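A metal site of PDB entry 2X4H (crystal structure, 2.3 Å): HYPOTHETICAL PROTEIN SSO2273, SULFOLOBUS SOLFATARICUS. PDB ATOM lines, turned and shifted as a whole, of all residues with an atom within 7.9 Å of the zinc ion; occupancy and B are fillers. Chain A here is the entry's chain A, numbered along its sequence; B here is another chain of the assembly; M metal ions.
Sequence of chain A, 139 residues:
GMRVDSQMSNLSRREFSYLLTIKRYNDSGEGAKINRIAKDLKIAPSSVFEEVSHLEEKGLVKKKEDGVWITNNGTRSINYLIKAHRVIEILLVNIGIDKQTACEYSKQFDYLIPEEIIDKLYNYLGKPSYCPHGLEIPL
The zinc ion is bound by a ring nitrogen (ND1) of His 54 (2.0 Å), the side-chain carboxylate (OE2) of Glu 15 (2.2 Å), the side-chain carboxylate (OE1) of Glu 65 of chain B (2.2 Å), the side-chain carboxylate (OE2) of Glu 51 (2.2 Å) and the side-chain carboxylate (OE2) of Glu 65 of chain B (2.4 Å).
The side-chain carboxylate of Glu 15 lies within salt-bridge range of the side-chain amino group of Lys 58.
The backbone NH (N) of Ser 12 is in hydrogen-bond range of the side-chain carboxylate (OE1) of Glu 15.
The guanidinium group (NH2) of Arg 14 lies close to the side-chain carboxylate (OE1) of Glu 65 of chain B.
The side-chain carboxylate (OE1) of Glu 51 is in salt-bridge range of the guanidinium group (NH2) of Arg 14, 2.7 Å away.
Within 4 Å of the zinc ion: Glu 15, Glu 51, His 54 and Glu 65 of chain B.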
ATOM      1  N   LEU A  11     -16.684  -4.717  -2.587  1.00  0.00           N
ATOM      2  CA  LEU A  11     -15.508  -4.856  -3.501  1.00  0.00           C
ATOM      3  C   LEU A  11     -15.860  -4.514  -4.944  1.00  0.00           C
ATOM      4  O   LEU A  11     -16.623  -5.227  -5.577  1.00  0.00           O
ATOM      5  CB  LEU A  11     -14.943  -6.289  -3.449  1.00  0.00           C
ATOM      6  CG  LEU A  11     -13.498  -6.492  -3.951  1.00  0.00           C
ATOM      7  CD1 LEU A  11     -12.536  -5.862  -2.990  1.00  0.00           C
ATOM      8  CD2 LEU A  11     -13.128  -7.953  -4.141  1.00  0.00           C
ATOM      9  N   SER A  12     -15.299  -3.418  -5.476  1.00  0.00           N
ATOM     10  CA  SER A  12     -15.431  -3.117  -6.911  1.00  0.00           C
ATOM     11  C   SER A  12     -14.486  -3.978  -7.768  1.00  0.00           C
ATOM     12  O   SER A  12     -13.517  -4.535  -7.271  1.00  0.00           O
ATOM     13  CB  SER A  12     -15.170  -1.640  -7.167  1.00  0.00           C
ATOM     14  OG  SER A  12     -13.780  -1.360  -7.041  1.00  0.00           O
ATOM     15  N   ARG A  14     -12.501  -2.858  -9.907  1.00  0.00           N
ATOM     16  CA  ARG A  14     -11.219  -2.180  -9.906  1.00  0.00           C
ATOM     17  C   ARG A  14     -10.401  -2.576  -8.682  1.00  0.00           C
ATOM     18  O   ARG A  14      -9.192  -2.877  -8.779  1.00  0.00           O
ATOM     19  CB  ARG A  14     -11.378  -0.669  -9.956  1.00  0.00           C
ATOM     20  CG  ARG A  14     -10.064   0.022 -10.373  1.00  0.00           C
ATOM     21  CD  ARG A  14     -10.303   1.486 -10.632  1.00  0.00           C
ATOM     22  NE  ARG A  14     -10.875   2.087  -9.434  1.00  0.00           N
ATOM     23  CZ  ARG A  14     -10.174   2.622  -8.434  1.00  0.00           C
ATOM     24  NH1 ARG A  14      -8.852   2.673  -8.490  1.00  0.00           N
ATOM     25  NH2 ARG A  14     -10.812   3.110  -7.383  1.00  0.00           N
ATOM     26  N   GLU A  15     -11.048  -2.579  -7.521  1.00  0.00           N
ATOM     27  CA  GLU A  15     -10.407  -3.074  -6.329  1.00  0.00           C
ATOM     28  C   GLU A  15      -9.995  -4.532  -6.539  1.00  0.00           C
ATOM     29  O   GLU A  15      -8.954  -4.947  -6.027  1.00  0.00           O
ATOM     30  CB  GLU A  15     -11.299  -2.934  -5.111  1.00  0.00           C
ATOM     31  CG  GLU A  15     -11.502  -1.479  -4.631  1.00  0.00           C
ATOM     32  CD  GLU A  15     -12.600  -1.393  -3.560  1.00  0.00           C
ATOM     33  OE1 GLU A  15     -13.466  -2.271  -3.530  1.00  0.00           O
ATOM     34  OE2 GLU A  15     -12.618  -0.469  -2.736  1.00  0.00           O
ATOM     35  N   TYR A  18      -6.590  -4.622  -8.206  1.00  0.00           N
ATOM     36  CA  TYR A  18      -5.560  -4.295  -7.234  1.00  0.00           C
ATOM     37  C   TYR A  18      -5.214  -5.492  -6.382  1.00  0.00           C
ATOM     38  O   TYR A  18      -4.041  -5.817  -6.193  1.00  0.00           O
ATOM     39  CB  TYR A  18      -6.043  -3.201  -6.289  1.00  0.00           C
ATOM     40  CG  TYR A  18      -5.846  -1.781  -6.769  1.00  0.00           C
ATOM     41  CD1 TYR A  18      -6.645  -1.236  -7.764  1.00  0.00           C
ATOM     42  CD2 TYR A  18      -4.876  -0.976  -6.181  1.00  0.00           C
ATOM     43  CE1 TYR A  18      -6.462   0.096  -8.182  1.00  0.00           C
ATOM     44  CE2 TYR A  18      -4.690   0.348  -6.585  1.00  0.00           C
ATOM     45  CZ  TYR A  18      -5.480   0.878  -7.582  1.00  0.00           C
ATOM     46  OH  TYR A  18      -5.292   2.190  -7.946  1.00  0.00           O
ATOM     47  N   GLU A  50      -3.755   6.239  -2.953  1.00  0.00           N
ATOM     48  CA  GLU A  50      -5.059   6.548  -2.354  1.00  0.00           C
ATOM     49  C   GLU A  50      -5.890   5.263  -2.163  1.00  0.00           C
ATOM     50  O   GLU A  50      -6.374   4.964  -1.086  1.00  0.00           O
ATOM     51  CB  GLU A  50      -5.805   7.627  -3.193  1.00  0.00           C
ATOM     52  CG  GLU A  50      -6.857   8.456  -2.391  1.00  0.00           C
ATOM     53  CD  GLU A  50      -7.247   9.806  -3.048  1.00  0.00           C
ATOM     54  OE1 GLU A  50      -8.440  10.203  -2.935  1.00  0.00           O
ATOM     55  OE2 GLU A  50      -6.387  10.483  -3.663  1.00  0.00           O
ATOM     56  N   GLU A  51      -5.996   4.475  -3.223  1.00  0.00           N
ATOM     57  CA  GLU A  51      -6.749   3.216  -3.206  1.00  0.00           C
ATOM     58  C   GLU A  51      -6.180   2.147  -2.228  1.00  0.00           C
ATOM     59  O   GLU A  51      -6.940   1.392  -1.607  1.00  0.00           O
ATOM     60  CB  GLU A  51      -6.795   2.669  -4.646  1.00  0.00           C
ATOM     61  CG  GLU A  51      -7.500   1.338  -4.843  1.00  0.00           C
ATOM     62  CD  GLU A  51      -8.966   1.415  -4.524  1.00  0.00           C
ATOM     63  OE1 GLU A  51      -9.778   1.545  -5.459  1.00  0.00           O
ATOM     64  OE2 GLU A  51      -9.306   1.357  -3.332  1.00  0.00           O
ATOM     65  N   VAL A  52      -4.860   2.075  -2.084  1.00  0.00           N
ATOM     66  CA  VAL A  52      -4.264   1.160  -1.109  1.00  0.00           C
ATOM     67  C   VAL A  52      -4.690   1.505   0.308  1.00  0.00           C
ATOM     68  O   VAL A  52      -5.092   0.617   1.060  1.00  0.00           O
ATOM     69  CB  VAL A  52      -2.729   1.070  -1.256  1.00  0.00           C
ATOM     70  CG1 VAL A  52      -2.038   0.634   0.064  1.00  0.00           C
ATOM     71  CG2 VAL A  52      -2.419   0.117  -2.398  1.00  0.00           C
ATOM     72  N   SER A  53      -4.664   2.786   0.670  1.00  0.00           N
ATOM     73  CA  SER A  53      -5.194   3.217   1.988  1.00  0.00           C
ATOM     74  C   SER A  53      -6.659   2.848   2.182  1.00  0.00           C
ATOM     75  O   SER A  53      -7.124   2.583   3.286  1.00  0.00           O
ATOM     76  CB  SER A  53      -5.059   4.734   2.143  1.00  0.00           C
ATOM     77  OG  SER A  53      -3.765   5.185   1.741  1.00  0.00           O
ATOM     78  N   HIS A  54      -7.418   2.856   1.097  1.00  0.00           N
ATOM     79  CA  HIS A  54      -8.835   2.514   1.163  1.00  0.00           C
ATOM     80  C   HIS A  54      -8.988   1.007   1.488  1.00  0.00           C
ATOM     81  O   HIS A  54      -9.789   0.601   2.357  1.00  0.00           O
ATOM     82  CB  HIS A  54      -9.502   2.909  -0.157  1.00  0.00           C
ATOM     83  CG  HIS A  54     -10.981   2.701  -0.160  1.00  0.00           C
ATOM     84  ND1 HIS A  54     -11.649   2.198  -1.250  1.00  0.00           N
ATOM     85  CD2 HIS A  54     -11.902   2.886   0.809  1.00  0.00           C
ATOM     86  CE1 HIS A  54     -12.934   2.090  -0.938  1.00  0.00           C
ATOM     87  NE2 HIS A  54     -13.112   2.510   0.298  1.00  0.00           N
ATOM     88  N   LEU A  55      -8.174   0.194   0.815  1.00  0.00           N
ATOM     89  CA  LEU A  55      -8.164  -1.242   1.001  1.00  0.00           C
ATOM     90  C   LEU A  55      -7.664  -1.595   2.429  1.00  0.00           C
ATOM     91  O   LEU A  55      -8.153  -2.551   3.055  1.00  0.00           O
ATOM     92  CB  LEU A  55      -7.303  -1.925  -0.084  1.00  0.00           C
ATOM     93  CG  LEU A  55      -7.843  -1.924  -1.540  1.00  0.00           C
ATOM     94  CD1 LEU A  55      -6.795  -2.452  -2.532  1.00  0.00           C
ATOM     95  CD2 LEU A  55      -9.131  -2.722  -1.677  1.00  0.00           C
ATOM     96  N   LYS A  58     -10.442  -1.042   4.887  1.00  0.00           N
ATOM     97  CA  LYS A  58     -11.428  -2.145   4.860  1.00  0.00           C
ATOM     98  C   LYS A  58     -10.838  -3.458   5.377  1.00  0.00           C
ATOM     99  O   LYS A  58     -11.497  -4.471   5.335  1.00  0.00           O
ATOM    100  CB  LYS A  58     -11.941  -2.353   3.433  1.00  0.00           C
ATOM    101  CG  LYS A  58     -12.776  -1.240   2.909  1.00  0.00           C
ATOM    102  CD  LYS A  58     -12.787  -1.189   1.383  1.00  0.00           C
ATOM    103  CE  LYS A  58     -13.813  -2.068   0.726  1.00  0.00           C
ATOM    104  NZ  LYS A  58     -14.162  -1.539  -0.617  1.00  0.00           N
ATOM    105  N   LEU A  60      -8.487  -5.355   4.110  1.00  0.00           N
ATOM    106  CA  LEU A  60      -8.217  -6.294   3.016  1.00  0.00           C
ATOM    107  C   LEU A  60      -6.724  -6.392   2.647  1.00  0.00           C
ATOM    108  O   LEU A  60      -6.301  -7.348   2.032  1.00  0.00           O
ATOM    109  CB  LEU A  60      -9.025  -5.871   1.785  1.00  0.00           C
ATOM    110  CG  LEU A  60     -10.551  -5.766   1.919  1.00  0.00           C
ATOM    111  CD1 LEU A  60     -11.167  -5.501   0.586  1.00  0.00           C
ATOM    112  CD2 LEU A  60     -11.121  -7.017   2.516  1.00  0.00           C
ATOM    113  N   GLU B  65     -14.361   6.841  -6.443  1.00  0.00           N
ATOM    114  CA  GLU B  65     -14.723   6.513  -5.059  1.00  0.00           C
ATOM    115  C   GLU B  65     -14.754   7.743  -4.162  1.00  0.00           C
ATOM    116  O   GLU B  65     -15.461   7.763  -3.163  1.00  0.00           O
ATOM    117  CB  GLU B  65     -13.704   5.551  -4.464  1.00  0.00           C
ATOM    118  CG  GLU B  65     -13.569   4.249  -5.201  1.00  0.00           C
ATOM    119  CD  GLU B  65     -12.743   3.258  -4.423  1.00  0.00           C
ATOM    120  OE1 GLU B  65     -12.793   2.059  -4.757  1.00  0.00           O
ATOM    121  OE2 GLU B  65     -12.077   3.677  -3.458  1.00  0.00           O
ATOM    122  N   ASP B  66     -13.926   8.713  -4.528  1.00  0.00           N
ATOM    123  CA  ASP B  66     -13.782   9.993  -3.837  1.00  0.00           C
ATOM    124  C   ASP B  66     -14.990  10.898  -4.061  1.00  0.00           C
ATOM    125  O   ASP B  66     -15.251  11.808  -3.277  1.00  0.00           O
ATOM    126  CB  ASP B  66     -12.523  10.695  -4.410  1.00  0.00           C
ATOM    127  CG  ASP B  66     -11.971  11.793  -3.497  1.00  0.00           C
ATOM    128  OD1 ASP B  66     -12.449  11.926  -2.343  1.00  0.00           O
ATOM    129  OD2 ASP B  66     -11.027  12.502  -3.919  1.00  0.00           O
HETATM  130 ZN    ZN M   1     -11.524   1.381  -3.048  1.00  0.00          ZN
